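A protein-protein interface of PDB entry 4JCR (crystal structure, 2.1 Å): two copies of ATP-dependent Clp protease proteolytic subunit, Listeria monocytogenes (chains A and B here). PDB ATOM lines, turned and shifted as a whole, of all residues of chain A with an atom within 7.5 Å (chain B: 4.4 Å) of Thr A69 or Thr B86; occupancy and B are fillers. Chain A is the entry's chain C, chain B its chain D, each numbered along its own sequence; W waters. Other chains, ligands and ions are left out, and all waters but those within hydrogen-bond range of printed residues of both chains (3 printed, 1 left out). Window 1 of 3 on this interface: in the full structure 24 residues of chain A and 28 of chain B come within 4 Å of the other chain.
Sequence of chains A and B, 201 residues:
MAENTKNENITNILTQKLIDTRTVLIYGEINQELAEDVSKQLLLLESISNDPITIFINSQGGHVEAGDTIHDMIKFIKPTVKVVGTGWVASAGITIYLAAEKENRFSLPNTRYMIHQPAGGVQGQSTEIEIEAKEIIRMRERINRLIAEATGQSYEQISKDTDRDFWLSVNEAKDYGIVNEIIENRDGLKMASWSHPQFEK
The side-chain amide oxygen of Asn B58 is in hydrogen-bond range of the side-chain hydroxyl of Thr A69 (2.6 Å).
The side-chain hydroxyl (OG1) of Thr B86 sits at hydrogen-bond distance from the side-chain hydroxyl (OG1) of Thr A69, at 2.8 Å.
NE2 of Gln A32 sits close to ND2 of Asn B58 (3.1 Å).
The side-chain hydroxyl (OH) of Tyr B27 sits at hydrogen-bond distance from the side-chain hydroxyl (OG) of Ser A39 (3.0 Å).
The side-chain amide nitrogen (NE2) of Gln A32 lies close to the indole nitrogen (NE1) of Trp B88 (3.4 Å).
The backbone carbonyl oxygen of Glu A65 lies close to the side-chain amide oxygen of Asn B58, 3.3 Å away.
O of Ala A35 sits at hydrogen-bond distance from OG of Ser A39, 2.9 Å away.
The side-chain hydroxyl (OG1) of Thr A69 lies within hydrogen-bond range of the backbone carbonyl oxygen (O) of Glu A65, 3.3 Å away.
The backbone NH of Gly B87 is in hydrogen-bond range of the side-chain hydroxyl of Thr B111 (3.4 Å).
The backbone carbonyl oxygen (O) of Leu B108 lies within hydrogen-bond range of the side-chain hydroxyl (OG1) of Thr B111 (2.8 Å).
The side-chain amide nitrogen of Asn B58 sits close to the indole nitrogen of Trp B88 (3.3 Å).
A ring nitrogen (NE2) of His A63 is in hydrogen-bond range of the side-chain carboxylate (OE1) of Glu A65, at 2.9 Å.
Gln A32 touches Tyr B27 (O to CD1, 3.7 Å).
O of Ala A35 touches CE1 of Tyr B27, 3.7 Å away.
N of Glu A36 touches CD1 of Tyr B27 (3.5 Å).
His A63 touches Trp B88 (NE2 to CZ2, 3.3 Å).
Gly B87 touches Glu A65 (CA to O, 3.5 Å).
Glu A65 touches Trp B88 (CG to CG, 3.5 Å).
Thr A69 touches Tyr B27.
N of Gly B87 touches OG1 of Thr A69 (3.6 Å).
CB of Leu B108 touches OD1 of Asp A72, 3.4 Å away.
Phe A76 touches Leu B108.
Printed residues of chain B within 4 Å of Ala A35: Tyr B27 (3.7 Å).
Printed residues of chain B within 4 Å of Glu A65: Asn B58 (3.3 Å), Gly B87 (3.5 Å) and Trp B88 (3.5 Å).
Thr A69 touches four residues of chain B.
Of the printed residues of chain B, Asp A72 touches Leu B108 (3.4 Å).
Ile B57 touches none of the printed residues of chain A.
Gly B85 touches none of the printed residues of chain A.
Of chain A, only Thr A69 comes within 4 Å of Thr B86.
Of the 22 printed residues of chain A, 9 touch a printed residue of chain B.
Printed residues of chain A that touch a printed residue of chain B: Gln A32, Ala A35, Glu A36, Ser A39, His A63, Glu A65, Thr A69, Asp A72 and Phe A76.
Of the 11 printed residues of chain B, 6 touch a printed residue of chain A.
Hydrophobic or aromatic side chains of chain B that line the printed part of chain A: Tyr B27, Trp B88 and Leu B108.
Among the printed residues, 16 pairs touch across the chains.
No position is printed for both chains.
Water W1 lies within hydrogen-bond range of OG1 of Thr B86 (2.7 Å), OD1 of Asp A72 (2.7 Å), N of Gly B87 (2.9 Å) and OG1 of Thr B111 (3.4 Å).
Water W2 lies within hydrogen-bond range of the backbone carbonyl oxygen (O) of Gly B87 (2.8 Å) and the side-chain carboxylate (OD1) of Asp A68 (2.8 Å).
Water W3 bridges the side-chain carboxylate of Glu A36 (2.9 Å) and the backbone NH of Tyr B27 (2.9 Å).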
ATOM      1  N   GLN A  32      19.146   9.906  27.296  1.00  0.00           N
ATOM      2  CA  GLN A  32      18.812  10.417  25.961  1.00  0.00           C
ATOM      3  C   GLN A  32      18.811   9.336  24.881  1.00  0.00           C
ATOM      4  O   GLN A  32      18.021   9.393  23.933  1.00  0.00           O
ATOM      5  CB  GLN A  32      19.738  11.573  25.579  1.00  0.00           C
ATOM      6  CG  GLN A  32      19.357  12.891  26.239  1.00  0.00           C
ATOM      7  CD  GLN A  32      20.495  13.898  26.261  1.00  0.00           C
ATOM      8  OE1 GLN A  32      21.621  13.574  26.640  1.00  0.00           O
ATOM      9  NE2 GLN A  32      20.198  15.134  25.865  1.00  0.00           N
ATOM     10  N   ALA A  35      15.611   7.407  25.429  1.00  0.00           N
ATOM     11  CA  ALA A  35      14.569   8.313  24.941  1.00  0.00           C
ATOM     12  C   ALA A  35      14.454   8.277  23.419  1.00  0.00           C
ATOM     13  O   ALA A  35      13.346   8.266  22.883  1.00  0.00           O
ATOM     14  CB  ALA A  35      14.812   9.733  25.431  1.00  0.00           C
ATOM     15  N   GLU A  36      15.595   8.241  22.731  1.00  0.00           N
ATOM     16  CA  GLU A  36      15.616   8.156  21.271  1.00  0.00           C
ATOM     17  C   GLU A  36      15.039   6.833  20.777  1.00  0.00           C
ATOM     18  O   GLU A  36      14.230   6.814  19.849  1.00  0.00           O
ATOM     19  CB  GLU A  36      17.033   8.357  20.725  1.00  0.00           C
ATOM     20  CG  GLU A  36      17.076   8.574  19.219  1.00  0.00           C
ATOM     21  CD  GLU A  36      18.486   8.620  18.659  1.00  0.00           C
ATOM     22  OE1 GLU A  36      19.399   9.128  19.346  1.00  0.00           O
ATOM     23  OE2 GLU A  36      18.677   8.151  17.517  1.00  0.00           O
ATOM     24  N   VAL A  38      12.956   4.802  22.416  1.00  0.00           N
ATOM     25  CA  VAL A  38      11.519   4.795  22.719  1.00  0.00           C
ATOM     26  C   VAL A  38      10.730   5.673  21.738  1.00  0.00           C
ATOM     27  O   VAL A  38       9.669   5.269  21.259  1.00  0.00           O
ATOM     28  CB  VAL A  38      11.248   5.208  24.187  1.00  0.00           C
ATOM     29  CG1 VAL A  38       9.754   5.357  24.455  1.00  0.00           C
ATOM     30  CG2 VAL A  38      11.856   4.192  25.145  1.00  0.00           C
ATOM     31  N   SER A  39      11.261   6.855  21.427  1.00  0.00           N
ATOM     32  CA  SER A  39      10.629   7.765  20.470  1.00  0.00           C
ATOM     33  C   SER A  39      10.456   7.130  19.097  1.00  0.00           C
ATOM     34  O   SER A  39       9.395   7.258  18.485  1.00  0.00           O
ATOM     35  CB  SER A  39      11.419   9.069  20.337  1.00  0.00           C
ATOM     36  OG  SER A  39      11.301   9.855  21.505  1.00  0.00           O
ATOM     37  N   LEU A  42       7.688   4.415  19.266  1.00  0.00           N
ATOM     38  CA  LEU A  42       6.359   5.029  19.340  1.00  0.00           C
ATOM     39  C   LEU A  42       5.923   5.672  18.021  1.00  0.00           C
ATOM     40  O   LEU A  42       4.766   5.539  17.617  1.00  0.00           O
ATOM     41  CB  LEU A  42       6.286   6.058  20.475  1.00  0.00           C
ATOM     42  CG  LEU A  42       6.459   5.574  21.921  1.00  0.00           C
ATOM     43  CD1 LEU A  42       6.526   6.771  22.860  1.00  0.00           C
ATOM     44  CD2 LEU A  42       5.351   4.616  22.338  1.00  0.00           C
ATOM     45  N   HIS A  63      17.929  10.541  33.748  1.00  0.00           N
ATOM     46  CA  HIS A  63      17.999  11.898  33.215  1.00  0.00           C
ATOM     47  C   HIS A  63      16.635  12.537  33.111  1.00  0.00           C
ATOM     48  O   HIS A  63      15.742  12.014  32.441  1.00  0.00           O
ATOM     49  CB  HIS A  63      18.718  11.877  31.866  1.00  0.00           C
ATOM     50  CG  HIS A  63      18.955  13.244  31.269  1.00  0.00           C
ATOM     51  ND1 HIS A  63      19.002  13.450  29.940  1.00  0.00           N
ATOM     52  CD2 HIS A  63      19.154  14.486  31.866  1.00  0.00           C
ATOM     53  CE1 HIS A  63      19.228  14.756  29.698  1.00  0.00           C
ATOM     54  NE2 HIS A  63      19.315  15.389  30.877  1.00  0.00           N
ATOM     55  N   VAL A  64      16.475  13.680  33.774  1.00  0.00           N
ATOM     56  CA  VAL A  64      15.186  14.382  33.862  1.00  0.00           C
ATOM     57  C   VAL A  64      14.611  14.752  32.488  1.00  0.00           C
ATOM     58  O   VAL A  64      13.467  14.412  32.176  1.00  0.00           O
ATOM     59  CB  VAL A  64      15.278  15.629  34.782  1.00  0.00           C
ATOM     60  CG1 VAL A  64      14.049  16.524  34.640  1.00  0.00           C
ATOM     61  CG2 VAL A  64      15.450  15.202  36.233  1.00  0.00           C
ATOM     62  N   GLU A  65      15.409  15.425  31.664  1.00  0.00           N
ATOM     63  CA  GLU A  65      14.953  15.880  30.353  1.00  0.00           C
ATOM     64  C   GLU A  65      14.644  14.724  29.401  1.00  0.00           C
ATOM     65  O   GLU A  65      13.791  14.851  28.522  1.00  0.00           O
ATOM     66  CB  GLU A  65      15.961  16.851  29.732  1.00  0.00           C
ATOM     67  CG  GLU A  65      15.988  18.223  30.399  1.00  0.00           C
ATOM     68  CD  GLU A  65      16.703  18.238  31.741  1.00  0.00           C
ATOM     69  OE1 GLU A  65      17.510  17.322  32.020  1.00  0.00           O
ATOM     70  OE2 GLU A  65      16.461  19.180  32.524  1.00  0.00           O
ATOM     71  N   ALA A  66      15.336  13.599  29.584  1.00  0.00           N
ATOM     72  CA  ALA A  66      15.065  12.395  28.807  1.00  0.00           C
ATOM     73  C   ALA A  66      13.700  11.818  29.187  1.00  0.00           C
ATOM     74  O   ALA A  66      12.958  11.349  28.325  1.00  0.00           O
ATOM     75  CB  ALA A  66      16.164  11.365  29.014  1.00  0.00           C
ATOM     76  N   GLY A  67      13.381  11.863  30.478  1.00  0.00           N
ATOM     77  CA  GLY A  67      12.070  11.452  30.978  1.00  0.00           C
ATOM     78  C   GLY A  67      10.955  12.361  30.484  1.00  0.00           C
ATOM     79  O   GLY A  67       9.864  11.886  30.160  1.00  0.00           O
ATOM     80  N   ASP A  68      11.240  13.665  30.427  1.00  0.00           N
ATOM     81  CA  ASP A  68      10.302  14.674  29.908  1.00  0.00           C
ATOM     82  C   ASP A  68       9.941  14.413  28.453  1.00  0.00           C
ATOM     83  O   ASP A  68       8.774  14.508  28.068  1.00  0.00           O
ATOM     84  CB  ASP A  68      10.890  16.083  30.034  1.00  0.00           C
ATOM     85  CG  ASP A  68      11.003  16.553  31.472  1.00  0.00           C
ATOM     86  OD1 ASP A  68      11.935  17.336  31.765  1.00  0.00           O
ATOM     87  OD2 ASP A  68      10.166  16.152  32.312  1.00  0.00           O
ATOM     88  N   THR A  69      10.953  14.086  27.653  1.00  0.00           N
ATOM     89  CA  THR A  69      10.772  13.771  26.242  1.00  0.00           C
ATOM     90  C   THR A  69       9.852  12.573  26.040  1.00  0.00           C
ATOM     91  O   THR A  69       8.940  12.628  25.217  1.00  0.00           O
ATOM     92  CB  THR A  69      12.124  13.530  25.532  1.00  0.00           C
ATOM     93  OG1 THR A  69      12.819  14.775  25.414  1.00  0.00           O
ATOM     94  CG2 THR A  69      11.918  12.953  24.139  1.00  0.00           C
ATOM     95  N   ILE A  70      10.100  11.501  26.788  1.00  0.00           N
ATOM     96  CA  ILE A  70       9.303  10.280  26.673  1.00  0.00           C
ATOM     97  C   ILE A  70       7.868  10.546  27.137  1.00  0.00           C
ATOM     98  O   ILE A  70       6.909  10.113  26.488  1.00  0.00           O
ATOM     99  CB  ILE A  70       9.942   9.097  27.441  1.00  0.00           C
ATOM    100  CG1 ILE A  70      11.345   8.794  26.889  1.00  0.00           C
ATOM    101  CG2 ILE A  70       9.063   7.853  27.351  1.00  0.00           C
ATOM    102  CD1 ILE A  70      12.181   7.866  27.751  1.00  0.00           C
ATOM    103  N   HIS A  71       7.738  11.268  28.250  1.00  0.00           N
ATOM    104  CA  HIS A  71       6.445  11.729  28.756  1.00  0.00           C
ATOM    105  C   HIS A  71       5.665  12.444  27.686  1.00  0.00           C
ATOM    106  O   HIS A  71       4.525  12.079  27.391  1.00  0.00           O
ATOM    107  CB  HIS A  71       6.648  12.639  29.965  1.00  0.00           C
ATOM    108  CG  HIS A  71       5.384  13.309  30.449  1.00  0.00           C
ATOM    109  ND1 HIS A  71       4.682  12.853  31.502  1.00  0.00           N
ATOM    110  CD2 HIS A  71       4.712  14.438  29.988  1.00  0.00           C
ATOM    111  CE1 HIS A  71       3.614  13.649  31.707  1.00  0.00           C
ATOM    112  NE2 HIS A  71       3.631  14.615  30.778  1.00  0.00           N
ATOM    113  N   ASP A  72       6.280  13.460  27.085  1.00  0.00           N
ATOM    114  CA  ASP A  72       5.614  14.286  26.079  1.00  0.00           C
ATOM    115  C   ASP A  72       5.336  13.546  24.775  1.00  0.00           C
ATOM    116  O   ASP A  72       4.323  13.804  24.123  1.00  0.00           O
ATOM    117  CB  ASP A  72       6.410  15.562  25.811  1.00  0.00           C
ATOM    118  CG  ASP A  72       6.272  16.584  26.925  1.00  0.00           C
ATOM    119  OD1 ASP A  72       6.876  17.671  26.815  1.00  0.00           O
ATOM    120  OD2 ASP A  72       5.562  16.306  27.911  1.00  0.00           O
ATOM    121  N   MET A  73       6.225  12.629  24.404  1.00  0.00           N
ATOM    122  CA  MET A  73       6.039  11.819  23.201  1.00  0.00           C
ATOM    123  C   MET A  73       4.855  10.861  23.330  1.00  0.00           C
ATOM    124  O   MET A  73       4.153  10.607  22.347  1.00  0.00           O
ATOM    125  CB  MET A  73       7.312  11.047  22.843  1.00  0.00           C
ATOM    126  CG  MET A  73       8.395  11.889  22.176  1.00  0.00           C
ATOM    127  SD  MET A  73       7.887  12.718  20.651  1.00  0.00           S
ATOM    128  CE  MET A  73       7.409  11.326  19.629  1.00  0.00           C
ATOM    129  N   ILE A  74       4.640  10.341  24.539  1.00  0.00           N
ATOM    130  CA  ILE A  74       3.485   9.495  24.834  1.00  0.00           C
ATOM    131  C   ILE A  74       2.178  10.272  24.628  1.00  0.00           C
ATOM    132  O   ILE A  74       1.239   9.762  24.015  1.00  0.00           O
ATOM    133  CB  ILE A  74       3.561   8.888  26.256  1.00  0.00           C
ATOM    134  CG1 ILE A  74       4.615   7.772  26.300  1.00  0.00           C
ATOM    135  CG2 ILE A  74       2.204   8.339  26.692  1.00  0.00           C
ATOM    136  CD1 ILE A  74       5.076   7.408  27.697  1.00  0.00           C
ATOM    137  N   LYS A  75       2.137  11.507  25.119  1.00  0.00           N
ATOM    138  CA  LYS A  75       0.963  12.364  24.952  1.00  0.00           C
ATOM    139  C   LYS A  75       0.836  12.918  23.534  1.00  0.00           C
ATOM    140  O   LYS A  75      -0.274  13.184  23.069  1.00  0.00           O
ATOM    141  CB  LYS A  75       0.967  13.503  25.973  1.00  0.00           C
ATOM    142  CG  LYS A  75       0.783  13.032  27.406  1.00  0.00           C
ATOM    143  CD  LYS A  75       0.453  14.181  28.341  1.00  0.00           C
ATOM    144  CE  LYS A  75       0.172  13.660  29.741  1.00  0.00           C
ATOM    145  NZ  LYS A  75      -0.260  14.726  30.686  1.00  0.00           N
ATOM    146  N   PHE A  76       1.969  13.076  22.852  1.00  0.00           N
ATOM    147  CA  PHE A  76       2.004  13.636  21.500  1.00  0.00           C
ATOM    148  C   PHE A  76       1.366  12.732  20.445  1.00  0.00           C
ATOM    149  O   PHE A  76       0.637  13.212  19.573  1.00  0.00           O
ATOM    150  CB  PHE A  76       3.442  13.985  21.093  1.00  0.00           C
ATOM    151  CG  PHE A  76       3.559  14.562  19.710  1.00  0.00           C
ATOM    152  CD1 PHE A  76       3.253  15.896  19.472  1.00  0.00           C
ATOM    153  CD2 PHE A  76       3.972  13.768  18.645  1.00  0.00           C
ATOM    154  CE1 PHE A  76       3.358  16.430  18.195  1.00  0.00           C
ATOM    155  CE2 PHE A  76       4.080  14.296  17.368  1.00  0.00           C
ATOM    156  CZ  PHE A  76       3.772  15.629  17.142  1.00  0.00           C
ATOM    157  N   THR A  95       7.697  10.030  36.049  1.00  0.00           N
ATOM    158  CA  THR A  95       7.272  11.048  35.085  1.00  0.00           C
ATOM    159  C   THR A  95       6.745  10.400  33.799  1.00  0.00           C
ATOM    160  O   THR A  95       5.705  10.808  33.272  1.00  0.00           O
ATOM    161  CB  THR A  95       8.417  12.034  34.767  1.00  0.00           C
ATOM    162  OG1 THR A  95       8.862  12.646  35.984  1.00  0.00           O
ATOM    163  CG2 THR A  95       7.955  13.125  33.802  1.00  0.00           C
ATOM    164  N   ILE A  96       7.460   9.384  33.319  1.00  0.00           N
ATOM    165  CA  ILE A  96       7.049   8.613  32.148  1.00  0.00           C
ATOM    166  C   ILE A  96       5.751   7.854  32.428  1.00  0.00           C
ATOM    167  O   ILE A  96       4.795   7.942  31.656  1.00  0.00           O
ATOM    168  CB  ILE A  96       8.150   7.621  31.712  1.00  0.00           C
ATOM    169  CG1 ILE A  96       9.393   8.382  31.232  1.00  0.00           C
ATOM    170  CG2 ILE A  96       7.629   6.669  30.639  1.00  0.00           C
ATOM    171  CD1 ILE A  96      10.638   7.530  31.136  1.00  0.00           C
ATOM    172  N   TYR B  27      18.936  13.810  19.485  1.00  0.00           N
ATOM    173  CA  TYR B  27      18.960  13.637  20.935  1.00  0.00           C
ATOM    174  C   TYR B  27      20.402  13.435  21.401  1.00  0.00           C
ATOM    175  O   TYR B  27      21.123  12.593  20.860  1.00  0.00           O
ATOM    176  CB  TYR B  27      18.135  12.413  21.363  1.00  0.00           C
ATOM    177  CG  TYR B  27      16.621  12.481  21.195  1.00  0.00           C
ATOM    178  CD1 TYR B  27      15.800  11.615  21.914  1.00  0.00           C
ATOM    179  CD2 TYR B  27      16.009  13.388  20.319  1.00  0.00           C
ATOM    180  CE1 TYR B  27      14.419  11.636  21.764  1.00  0.00           C
ATOM    181  CE2 TYR B  27      14.628  13.420  20.167  1.00  0.00           C
ATOM    182  CZ  TYR B  27      13.838  12.544  20.892  1.00  0.00           C
ATOM    183  OH  TYR B  27      12.468  12.564  20.753  1.00  0.00           O
ATOM    184  N   ILE B  57      14.236  17.709  18.657  1.00  0.00           N
ATOM    185  CA  ILE B  57      15.536  18.027  19.242  1.00  0.00           C
ATOM    186  C   ILE B  57      15.479  17.996  20.766  1.00  0.00           C
ATOM    187  O   ILE B  57      14.673  18.699  21.385  1.00  0.00           O
ATOM    188  CB  ILE B  57      16.072  19.408  18.786  1.00  0.00           C
ATOM    189  CG1 ILE B  57      15.843  19.617  17.285  1.00  0.00           C
ATOM    190  CG2 ILE B  57      17.557  19.544  19.129  1.00  0.00           C
ATOM    191  CD1 ILE B  57      16.015  21.050  16.816  1.00  0.00           C
ATOM    192  N   ASN B  58      16.337  17.160  21.347  1.00  0.00           N
ATOM    193  CA  ASN B  58      16.580  17.120  22.784  1.00  0.00           C
ATOM    194  C   ASN B  58      18.098  17.144  22.973  1.00  0.00           C
ATOM    195  O   ASN B  58      18.755  16.104  22.908  1.00  0.00           O
ATOM    196  CB  ASN B  58      15.963  15.852  23.403  1.00  0.00           C
ATOM    197  CG  ASN B  58      16.207  15.734  24.909  1.00  0.00           C
ATOM    198  OD1 ASN B  58      15.367  15.217  25.646  1.00  0.00           O
ATOM    199  ND2 ASN B  58      17.358  16.195  25.366  1.00  0.00           N
ATOM    200  N   VAL B  84      10.717  20.530  16.562  1.00  0.00           N
ATOM    201  CA  VAL B  84       9.971  20.381  17.803  1.00  0.00           C
ATOM    202  C   VAL B  84      10.971  20.221  18.945  1.00  0.00           C
ATOM    203  O   VAL B  84      11.687  19.221  19.016  1.00  0.00           O
ATOM    204  CB  VAL B  84       8.995  19.179  17.766  1.00  0.00           C
ATOM    205  CG1 VAL B  84       8.281  19.023  19.102  1.00  0.00           C
ATOM    206  CG2 VAL B  84       7.980  19.330  16.642  1.00  0.00           C
ATOM    207  N   GLY B  85      11.026  21.223  19.819  1.00  0.00           N
ATOM    208  CA  GLY B  85      11.882  21.176  20.999  1.00  0.00           C
ATOM    209  C   GLY B  85      11.267  20.289  22.063  1.00  0.00           C
ATOM    210  O   GLY B  85      10.051  20.324  22.281  1.00  0.00           O
ATOM    211  N   THR B  86      12.105  19.491  22.719  1.00  0.00           N
ATOM    212  CA  THR B  86      11.642  18.545  23.734  1.00  0.00           C
ATOM    213  C   THR B  86      12.706  18.264  24.806  1.00  0.00           C
ATOM    214  O   THR B  86      13.870  18.029  24.484  1.00  0.00           O
ATOM    215  CB  THR B  86      11.105  17.239  23.095  1.00  0.00           C
ATOM    216  OG1 THR B  86      10.784  16.289  24.118  1.00  0.00           O
ATOM    217  CG2 THR B  86      12.108  16.624  22.104  1.00  0.00           C
ATOM    218  N   GLY B  87      12.298  18.304  26.074  1.00  0.00           N
ATOM    219  CA  GLY B  87      13.209  18.090  27.207  1.00  0.00           C
ATOM    220  C   GLY B  87      14.051  19.320  27.484  1.00  0.00           C
ATOM    221  O   GLY B  87      13.746  20.097  28.383  1.00  0.00           O
ATOM    222  N   TRP B  88      15.126  19.485  26.719  1.00  0.00           N
ATOM    223  CA  TRP B  88      15.855  20.755  26.687  1.00  0.00           C
ATOM    224  C   TRP B  88      16.480  21.028  25.353  1.00  0.00           C
ATOM    225  O   TRP B  88      16.741  20.109  24.578  1.00  0.00           O
ATOM    226  CB  TRP B  88      16.885  20.888  27.818  1.00  0.00           C
ATOM    227  CG  TRP B  88      17.927  19.791  27.936  1.00  0.00           C
ATOM    228  CD1 TRP B  88      18.175  18.736  27.059  1.00  0.00           C
ATOM    229  CD2 TRP B  88      18.930  19.637  29.003  1.00  0.00           C
ATOM    230  NE1 TRP B  88      19.214  17.958  27.509  1.00  0.00           N
ATOM    231  CE2 TRP B  88      19.712  18.444  28.666  1.00  0.00           C
ATOM    232  CE3 TRP B  88      19.238  20.339  30.165  1.00  0.00           C
ATOM    233  CZ2 TRP B  88      20.755  17.994  29.470  1.00  0.00           C
ATOM    234  CZ3 TRP B  88      20.291  19.875  30.967  1.00  0.00           C
ATOM    235  CH2 TRP B  88      21.028  18.731  30.626  1.00  0.00           C
ATOM    236  N   VAL B  89      16.689  22.311  25.071  1.00  0.00           N
ATOM    237  CA  VAL B  89      17.377  22.760  23.869  1.00  0.00           C
ATOM    238  C   VAL B  89      18.303  23.892  24.307  1.00  0.00           C
ATOM    239  O   VAL B  89      17.840  24.964  24.710  1.00  0.00           O
ATOM    240  CB  VAL B  89      16.398  23.241  22.768  1.00  0.00           C
ATOM    241  CG1 VAL B  89      17.147  23.547  21.483  1.00  0.00           C
ATOM    242  CG2 VAL B  89      15.316  22.197  22.496  1.00  0.00           C
ATOM    243  N   LEU B 108       7.274  20.955  22.647  1.00  0.00           N
ATOM    244  CA  LEU B 108       6.484  20.138  23.559  1.00  0.00           C
ATOM    245  C   LEU B 108       6.467  20.839  24.925  1.00  0.00           C
ATOM    246  O   LEU B 108       7.370  21.624  25.216  1.00  0.00           O
ATOM    247  CB  LEU B 108       7.053  18.718  23.635  1.00  0.00           C
ATOM    248  CG  LEU B 108       6.451  17.600  22.762  1.00  0.00           C
ATOM    249  CD1 LEU B 108       5.556  18.087  21.628  1.00  0.00           C
ATOM    250  CD2 LEU B 108       7.528  16.672  22.226  1.00  0.00           C
ATOM    251  N   THR B 111       9.784  21.341  28.301  1.00  0.00           N
ATOM    252  CA  THR B 111      11.034  21.688  27.634  1.00  0.00           C
ATOM    253  C   THR B 111      11.543  23.009  28.190  1.00  0.00           C
ATOM    254  O   THR B 111      10.773  23.961  28.344  1.00  0.00           O
ATOM    255  CB  THR B 111      10.834  21.869  26.109  1.00  0.00           C
ATOM    256  OG1 THR B 111      10.066  20.782  25.583  1.00  0.00           O
ATOM    257  CG2 THR B 111      12.175  21.938  25.376  1.00  0.00           C
HETATM  258  O   HOH W   1       9.507  17.509  26.160  1.00  0.00           O
HETATM  259  O   HOH W   2      12.544  19.932  30.859  1.00  0.00           O
HETATM  260  O   HOH W   3      19.835  11.547  17.877  1.00  0.00           O
